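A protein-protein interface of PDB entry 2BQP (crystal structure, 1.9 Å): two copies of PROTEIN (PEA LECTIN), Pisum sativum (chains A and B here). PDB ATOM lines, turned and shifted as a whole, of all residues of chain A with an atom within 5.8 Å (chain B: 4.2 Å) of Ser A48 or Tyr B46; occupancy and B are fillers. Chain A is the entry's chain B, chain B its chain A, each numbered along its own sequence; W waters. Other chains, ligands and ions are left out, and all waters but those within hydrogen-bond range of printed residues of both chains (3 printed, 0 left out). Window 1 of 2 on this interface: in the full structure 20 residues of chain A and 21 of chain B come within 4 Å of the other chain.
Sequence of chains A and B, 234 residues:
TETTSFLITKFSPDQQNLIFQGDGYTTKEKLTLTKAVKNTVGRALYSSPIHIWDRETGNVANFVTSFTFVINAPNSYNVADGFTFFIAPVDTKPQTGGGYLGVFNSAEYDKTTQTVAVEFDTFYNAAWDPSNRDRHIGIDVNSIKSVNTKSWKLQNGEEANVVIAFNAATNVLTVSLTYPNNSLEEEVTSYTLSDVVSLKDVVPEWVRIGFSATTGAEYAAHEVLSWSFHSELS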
ATOM      1  N   THR A   4      -9.148  -0.754   8.985  1.00  0.00           N
ATOM      2  CA  THR A   4      -9.886  -1.519   8.004  1.00  0.00           C
ATOM      3  C   THR A   4      -8.880  -2.177   7.090  1.00  0.00           C
ATOM      4  O   THR A   4      -7.976  -1.501   6.570  1.00  0.00           O
ATOM      5  CB  THR A   4     -10.750  -0.618   7.155  1.00  0.00           C
ATOM      6  OG1 THR A   4     -11.665   0.096   7.983  1.00  0.00           O
ATOM      7  CG2 THR A   4     -11.494  -1.418   6.110  1.00  0.00           C
ATOM      8  N   ASN A  17     -18.265  -8.204  -2.065  1.00  0.00           N
ATOM      9  CA  ASN A  17     -17.749  -7.129  -1.241  1.00  0.00           C
ATOM     10  C   ASN A  17     -17.237  -5.933  -2.063  1.00  0.00           C
ATOM     11  O   ASN A  17     -16.728  -4.941  -1.508  1.00  0.00           O
ATOM     12  CB  ASN A  17     -16.720  -7.633  -0.222  1.00  0.00           C
ATOM     13  CG  ASN A  17     -15.624  -8.430  -0.844  1.00  0.00           C
ATOM     14  OD1 ASN A  17     -15.694  -8.822  -2.010  1.00  0.00           O
ATOM     15  ND2 ASN A  17     -14.593  -8.687  -0.069  1.00  0.00           N
ATOM     16  N   ILE A  19     -18.284  -3.021  -5.245  1.00  0.00           N
ATOM     17  CA  ILE A  19     -19.397  -2.346  -5.921  1.00  0.00           C
ATOM     18  C   ILE A  19     -18.893  -2.016  -7.342  1.00  0.00           C
ATOM     19  O   ILE A  19     -17.892  -1.339  -7.505  1.00  0.00           O
ATOM     20  CB  ILE A  19     -19.799  -1.030  -5.207  1.00  0.00           C
ATOM     21  CG1 ILE A  19     -20.343  -1.335  -3.818  1.00  0.00           C
ATOM     22  CG2 ILE A  19     -20.826  -0.256  -6.047  1.00  0.00           C
ATOM     23  CD1 ILE A  19     -20.336  -0.141  -2.925  1.00  0.00           C
ATOM     24  N   TYR A  46     -14.643  -0.670  -3.006  1.00  0.00           N
ATOM     25  CA  TYR A  46     -14.758  -1.627  -1.908  1.00  0.00           C
ATOM     26  C   TYR A  46     -16.070  -1.218  -1.241  1.00  0.00           C
ATOM     27  O   TYR A  46     -16.277  -0.042  -0.962  1.00  0.00           O
ATOM     28  CB  TYR A  46     -13.597  -1.498  -0.928  1.00  0.00           C
ATOM     29  CG  TYR A  46     -13.639  -2.522   0.204  1.00  0.00           C
ATOM     30  CD1 TYR A  46     -13.697  -3.889  -0.068  1.00  0.00           C
ATOM     31  CD2 TYR A  46     -13.660  -2.111   1.533  1.00  0.00           C
ATOM     32  CE1 TYR A  46     -13.771  -4.821   0.958  1.00  0.00           C
ATOM     33  CE2 TYR A  46     -13.749  -3.034   2.578  1.00  0.00           C
ATOM     34  CZ  TYR A  46     -13.801  -4.387   2.288  1.00  0.00           C
ATOM     35  OH  TYR A  46     -13.881  -5.314   3.319  1.00  0.00           O
ATOM     36  N   SER A  47     -16.963  -2.176  -1.001  1.00  0.00           N
ATOM     37  CA  SER A  47     -18.266  -1.871  -0.408  1.00  0.00           C
ATOM     38  C   SER A  47     -18.268  -1.001   0.847  1.00  0.00           C
ATOM     39  O   SER A  47     -19.040  -0.055   0.953  1.00  0.00           O
ATOM     40  CB  SER A  47     -19.068  -3.156  -0.151  1.00  0.00           C
ATOM     41  OG  SER A  47     -18.303  -4.075   0.607  1.00  0.00           O
ATOM     42  N   SER A  48     -17.401  -1.298   1.800  1.00  0.00           N
ATOM     43  CA  SER A  48     -17.402  -0.518   3.018  1.00  0.00           C
ATOM     44  C   SER A  48     -16.744   0.861   2.992  1.00  0.00           C
ATOM     45  O   SER A  48     -15.636   1.008   2.481  1.00  0.00           O
ATOM     46  CB  SER A  48     -16.719  -1.309   4.127  1.00  0.00           C
ATOM     47  OG  SER A  48     -16.672  -0.522   5.305  1.00  0.00           O
ATOM     48  N   PRO A  49     -17.436   1.898   3.508  1.00  0.00           N
ATOM     49  CA  PRO A  49     -16.860   3.242   3.556  1.00  0.00           C
ATOM     50  C   PRO A  49     -15.643   3.144   4.521  1.00  0.00           C
ATOM     51  O   PRO A  49     -15.655   2.323   5.458  1.00  0.00           O
ATOM     52  CB  PRO A  49     -17.986   4.053   4.200  1.00  0.00           C
ATOM     53  CG  PRO A  49     -19.212   3.386   3.644  1.00  0.00           C
ATOM     54  CD  PRO A  49     -18.885   1.937   3.784  1.00  0.00           C
ATOM     55  N   ILE A  50     -14.605   3.950   4.278  1.00  0.00           N
ATOM     56  CA  ILE A  50     -13.383   3.975   5.099  1.00  0.00           C
ATOM     57  C   ILE A  50     -13.307   5.288   5.879  1.00  0.00           C
ATOM     58  O   ILE A  50     -13.666   6.342   5.352  1.00  0.00           O
ATOM     59  CB  ILE A  50     -12.122   3.918   4.215  1.00  0.00           C
ATOM     60  CG1 ILE A  50     -12.134   2.694   3.292  1.00  0.00           C
ATOM     61  CG2 ILE A  50     -10.876   3.958   5.065  1.00  0.00           C
ATOM     62  CD1 ILE A  50     -12.094   1.372   3.995  1.00  0.00           C
ATOM     63  N   VAL A 207     -14.923   8.002   3.087  1.00  0.00           N
ATOM     64  CA  VAL A 207     -14.705   7.891   1.663  1.00  0.00           C
ATOM     65  C   VAL A 207     -14.869   6.445   1.203  1.00  0.00           C
ATOM     66  O   VAL A 207     -15.078   5.536   2.016  1.00  0.00           O
ATOM     67  CB  VAL A 207     -13.238   8.280   1.317  1.00  0.00           C
ATOM     68  CG1 VAL A 207     -12.968   9.724   1.632  1.00  0.00           C
ATOM     69  CG2 VAL A 207     -12.253   7.347   2.059  1.00  0.00           C
ATOM     70  N   ARG A 208     -14.823   6.239  -0.104  1.00  0.00           N
ATOM     71  CA  ARG A 208     -14.838   4.890  -0.657  1.00  0.00           C
ATOM     72  C   ARG A 208     -13.619   4.918  -1.557  1.00  0.00           C
ATOM     73  O   ARG A 208     -13.302   5.969  -2.107  1.00  0.00           O
ATOM     74  CB  ARG A 208     -16.101   4.570  -1.474  1.00  0.00           C
ATOM     75  CG  ARG A 208     -17.204   3.883  -0.657  1.00  0.00           C
ATOM     76  CD  ARG A 208     -18.159   3.104  -1.541  1.00  0.00           C
ATOM     77  NE  ARG A 208     -19.050   2.270  -0.733  1.00  0.00           N
ATOM     78  CZ  ARG A 208     -20.232   2.664  -0.265  1.00  0.00           C
ATOM     79  NH1 ARG A 208     -20.696   3.873  -0.540  1.00  0.00           N
ATOM     80  NH2 ARG A 208     -20.921   1.879   0.550  1.00  0.00           N
ATOM     81  N   ILE A 209     -12.908   3.799  -1.645  1.00  0.00           N
ATOM     82  CA  ILE A 209     -11.727   3.686  -2.483  1.00  0.00           C
ATOM     83  C   ILE A 209     -11.977   2.688  -3.591  1.00  0.00           C
ATOM     84  O   ILE A 209     -12.756   1.759  -3.430  1.00  0.00           O
ATOM     85  CB  ILE A 209     -10.523   3.168  -1.693  1.00  0.00           C
ATOM     86  CG1 ILE A 209     -10.841   1.761  -1.152  1.00  0.00           C
ATOM     87  CG2 ILE A 209     -10.181   4.155  -0.557  1.00  0.00           C
ATOM     88  CD1 ILE A 209      -9.728   1.112  -0.420  1.00  0.00           C
ATOM     89  N   PHE B   6     -11.318  -5.568  10.664  1.00  0.00           N
ATOM     90  CA  PHE B   6     -11.608  -4.216  11.123  1.00  0.00           C
ATOM     91  C   PHE B   6     -11.486  -4.134  12.631  1.00  0.00           C
ATOM     92  O   PHE B   6     -11.470  -5.151  13.310  1.00  0.00           O
ATOM     93  CB  PHE B   6     -12.957  -3.668  10.621  1.00  0.00           C
ATOM     94  CG  PHE B   6     -14.149  -4.406  11.124  1.00  0.00           C
ATOM     95  CD1 PHE B   6     -14.757  -4.040  12.324  1.00  0.00           C
ATOM     96  CD2 PHE B   6     -14.689  -5.450  10.386  1.00  0.00           C
ATOM     97  CE1 PHE B   6     -15.897  -4.712  12.781  1.00  0.00           C
ATOM     98  CE2 PHE B   6     -15.816  -6.117  10.831  1.00  0.00           C
ATOM     99  CZ  PHE B   6     -16.419  -5.747  12.026  1.00  0.00           C
ATOM    100  N   ASN B  17     -19.522   2.855   8.459  1.00  0.00           N
ATOM    101  CA  ASN B  17     -19.216   1.487   8.026  1.00  0.00           C
ATOM    102  C   ASN B  17     -20.115   0.423   8.711  1.00  0.00           C
ATOM    103  O   ASN B  17     -19.891  -0.786   8.612  1.00  0.00           O
ATOM    104  CB  ASN B  17     -17.730   1.162   8.153  1.00  0.00           C
ATOM    105  CG  ASN B  17     -17.158   1.435   9.530  1.00  0.00           C
ATOM    106  OD1 ASN B  17     -15.980   1.170   9.765  1.00  0.00           O
ATOM    107  ND2 ASN B  17     -17.950   1.994  10.428  1.00  0.00           N
ATOM    108  N   LEU B  18     -21.160   0.898   9.381  1.00  0.00           N
ATOM    109  CA  LEU B  18     -22.131   0.048  10.053  1.00  0.00           C
ATOM    110  C   LEU B  18     -23.500   0.340   9.454  1.00  0.00           C
ATOM    111  O   LEU B  18     -23.752   1.450   8.989  1.00  0.00           O
ATOM    112  CB  LEU B  18     -22.179   0.373  11.540  1.00  0.00           C
ATOM    113  CG  LEU B  18     -21.421  -0.539  12.513  1.00  0.00           C
ATOM    114  CD1 LEU B  18     -20.183  -1.112  11.902  1.00  0.00           C
ATOM    115  CD2 LEU B  18     -21.101   0.243  13.742  1.00  0.00           C
ATOM    116  N   LEU B  45     -25.083  -3.799  11.725  1.00  0.00           N
ATOM    117  CA  LEU B  45     -24.413  -4.726  10.821  1.00  0.00           C
ATOM    118  C   LEU B  45     -23.168  -4.055  10.278  1.00  0.00           C
ATOM    119  O   LEU B  45     -23.172  -2.846  10.102  1.00  0.00           O
ATOM    120  CB  LEU B  45     -25.327  -5.023   9.620  1.00  0.00           C
ATOM    121  CG  LEU B  45     -26.740  -5.623   9.726  1.00  0.00           C
ATOM    122  CD1 LEU B  45     -26.654  -7.091  10.039  1.00  0.00           C
ATOM    123  CD2 LEU B  45     -27.571  -4.895  10.754  1.00  0.00           C
ATOM    124  N   TYR B  46     -22.098  -4.810  10.048  1.00  0.00           N
ATOM    125  CA  TYR B  46     -20.907  -4.224   9.442  1.00  0.00           C
ATOM    126  C   TYR B  46     -21.301  -4.093   7.968  1.00  0.00           C
ATOM    127  O   TYR B  46     -21.890  -5.017   7.403  1.00  0.00           O
ATOM    128  CB  TYR B  46     -19.723  -5.158   9.570  1.00  0.00           C
ATOM    129  CG  TYR B  46     -18.482  -4.587   8.966  1.00  0.00           C
ATOM    130  CD1 TYR B  46     -17.942  -3.381   9.437  1.00  0.00           C
ATOM    131  CD2 TYR B  46     -17.847  -5.235   7.921  1.00  0.00           C
ATOM    132  CE1 TYR B  46     -16.793  -2.834   8.867  1.00  0.00           C
ATOM    133  CE2 TYR B  46     -16.695  -4.705   7.353  1.00  0.00           C
ATOM    134  CZ  TYR B  46     -16.175  -3.510   7.828  1.00  0.00           C
ATOM    135  OH  TYR B  46     -15.018  -3.028   7.269  1.00  0.00           O
ATOM    136  N   SER B  47     -20.951  -2.985   7.325  1.00  0.00           N
ATOM    137  CA  SER B  47     -21.366  -2.775   5.945  1.00  0.00           C
ATOM    138  C   SER B  47     -20.929  -3.773   4.897  1.00  0.00           C
ATOM    139  O   SER B  47     -21.701  -4.126   4.014  1.00  0.00           O
ATOM    140  CB  SER B  47     -20.986  -1.371   5.482  1.00  0.00           C
ATOM    141  OG  SER B  47     -19.591  -1.187   5.624  1.00  0.00           O
ATOM    142  N   SER B  48     -19.705  -4.252   4.970  1.00  0.00           N
ATOM    143  CA  SER B  48     -19.282  -5.177   3.943  1.00  0.00           C
ATOM    144  C   SER B  48     -19.649  -6.655   4.115  1.00  0.00           C
ATOM    145  O   SER B  48     -19.625  -7.181   5.230  1.00  0.00           O
ATOM    146  CB  SER B  48     -17.767  -5.060   3.726  1.00  0.00           C
ATOM    147  OG  SER B  48     -17.310  -5.997   2.766  1.00  0.00           O
ATOM    148  N   ARG B 208     -23.505 -11.218   6.299  1.00  0.00           N
ATOM    149  CA  ARG B 208     -23.286  -9.961   6.996  1.00  0.00           C
ATOM    150  C   ARG B 208     -23.296 -10.343   8.472  1.00  0.00           C
ATOM    151  O   ARG B 208     -24.004 -11.265   8.880  1.00  0.00           O
ATOM    152  CB  ARG B 208     -24.360  -8.916   6.694  1.00  0.00           C
ATOM    153  CG  ARG B 208     -23.962  -7.996   5.540  1.00  0.00           C
ATOM    154  CD  ARG B 208     -24.542  -6.616   5.690  1.00  0.00           C
ATOM    155  NE  ARG B 208     -24.080  -5.724   4.630  1.00  0.00           N
ATOM    156  CZ  ARG B 208     -24.799  -5.368   3.566  1.00  0.00           C
ATOM    157  NH1 ARG B 208     -26.036  -5.831   3.406  1.00  0.00           N
ATOM    158  NH2 ARG B 208     -24.274  -4.537   2.658  1.00  0.00           N
ATOM    159  N   ILE B 209     -22.479  -9.682   9.264  1.00  0.00           N
ATOM    160  CA  ILE B 209     -22.399 -10.001  10.684  1.00  0.00           C
ATOM    161  C   ILE B 209     -22.835  -8.770  11.461  1.00  0.00           C
ATOM    162  O   ILE B 209     -22.686  -7.652  10.973  1.00  0.00           O
ATOM    163  CB  ILE B 209     -20.949 -10.384  11.053  1.00  0.00           C
ATOM    164  CG1 ILE B 209     -20.008  -9.238  10.655  1.00  0.00           C
ATOM    165  CG2 ILE B 209     -20.544 -11.631  10.302  1.00  0.00           C
ATOM    166  CD1 ILE B 209     -18.601  -9.449  11.039  1.00  0.00           C
ATOM    167  N   TRP B 227     -15.215  -3.261  19.038  1.00  0.00           N
ATOM    168  CA  TRP B 227     -15.476  -4.419  18.208  1.00  0.00           C
ATOM    169  C   TRP B 227     -14.382  -4.656  17.177  1.00  0.00           C
ATOM    170  O   TRP B 227     -13.930  -3.726  16.515  1.00  0.00           O
ATOM    171  CB  TRP B 227     -16.836  -4.211  17.500  1.00  0.00           C
ATOM    172  CG  TRP B 227     -17.368  -5.374  16.671  1.00  0.00           C
ATOM    173  CD1 TRP B 227     -17.046  -6.694  16.802  1.00  0.00           C
ATOM    174  CD2 TRP B 227     -18.347  -5.306  15.615  1.00  0.00           C
ATOM    175  NE1 TRP B 227     -17.766  -7.447  15.909  1.00  0.00           N
ATOM    176  CE2 TRP B 227     -18.574  -6.625  15.171  1.00  0.00           C
ATOM    177  CE3 TRP B 227     -19.058  -4.250  15.004  1.00  0.00           C
ATOM    178  CZ2 TRP B 227     -19.489  -6.934  14.143  1.00  0.00           C
ATOM    179  CZ3 TRP B 227     -19.966  -4.559  13.984  1.00  0.00           C
ATOM    180  CH2 TRP B 227     -20.172  -5.890  13.570  1.00  0.00           C
HETATM  181  O   HOH W   1     -14.448  -0.175   7.501  1.00  0.00           O
HETATM  182  O   HOH W   2     -13.105  -4.660   5.957  1.00  0.00           O
HETATM  183  O   HOH W   3     -15.138  -7.763   2.598  1.00  0.00           O
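Among the printed residues, merely in contact across the chains: Asn A17 with Ser B48 (3.5 Å), Ser A48 with Asn B17 (3.5 Å), Tyr A46 with Ser B48 (3.5 Å), Ser A48 with Tyr B46 (3.6 Å), Pro A49 with Asn B17 (3.6 Å), Pro A49 with Ser B47 (3.7 Å) and Ser A48 with Ser B48 (3.9 Å).
The side-chain hydroxyl of Ser B47 is in hydrogen-bond range of the side-chain hydroxyl of Ser A48.
OG of Ser B48 lies within hydrogen-bond range of OG of Ser A47.
Hydrophobic or aromatic side chains of chain A that line the printed part of chain B: Tyr A46 and Pro A49.
Of the 10 printed residues of chain B, 4 touch a printed residue of chain A.
Hydrophobic or aromatic side chains of chain B within 4 Å of the printed part of chain A: Tyr B46.
Along chain B the printed residues that touch a printed residue of chain A span positions 17 to 48.
Among the printed residues, no Asp or Glu carboxylate lies within 4 Å of a Lys or Arg side-chain nitrogen of the other chain.
Ser A48 touches just these residues of chain B: Asn B17 (3.5 Å), Tyr B46 (3.6 Å), Ser B47 (3.0 Å) and Ser B48 (3.9 Å).
Of the printed residues of chain A, Tyr B46 touches Ser A48 (3.6 Å).
Of the printed residues of chain A, Ser B47 touches Ser A48 (3.0 Å) and Pro A49 (3.7 Å).
Printed residues of chain A within 4 Å of Ser B48: Asn A17, Tyr A46, Ser A47 and Ser A48.
The nearest printed residue of chain B that does not touch Pro A49 is Tyr B46 (5.7 Å).
Asn A17 touches Ser B48, and with the chains exchanged Ser A48 touches Asn B17.
Tyr A46 touches Ser B48, and with the chains exchanged Ser A48 touches Tyr B46.
Ser A47 touches Ser B48, and with the chains exchanged Ser A48 touches Ser B47.
Ser B48 touches its own counterpart, Ser A48.
Positions printed for both chains: 17, 46, 47, 48, 208 and 209.
Of the 9 pairs that touch across the chains among the printed residues, 7 have their exchanged pair printed and touching as well.
Water W3 lies within hydrogen-bond range of the side-chain hydroxyl of Ser B48 (2.8 Å), the side-chain hydroxyl of Tyr A46 (2.8 Å) and the side-chain amide nitrogen of Asn A17 (2.9 Å).
Water W2 bridges the side-chain hydroxyl (OH) of Tyr A46 (2.8 Å) and the side-chain hydroxyl (OH) of Tyr B46 (2.8 Å).
Water W1 lies within hydrogen-bond range of OG1 of Thr A4, OH of Tyr B46, OD1 of Asn B17, OG of Ser A48 and O of Pro A49.
O of Asn B17 sits at hydrogen-bond distance from N of Ser B47 (2.8 Å).
N of Tyr B46 sits at hydrogen-bond distance from O of Ile B209.
O of Ser B47 is in hydrogen-bond range of NE of Arg B208 (2.9 Å).
O of Asn A17 sits at hydrogen-bond distance from OG of Ser A47 (2.8 Å).
The backbone NH of Tyr A46 is in hydrogen-bond range of the backbone carbonyl oxygen of Ile A209, 3.1 Å away.
O of Ser A47 lies within hydrogen-bond range of NH2 of Arg A208 (2.7 Å).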
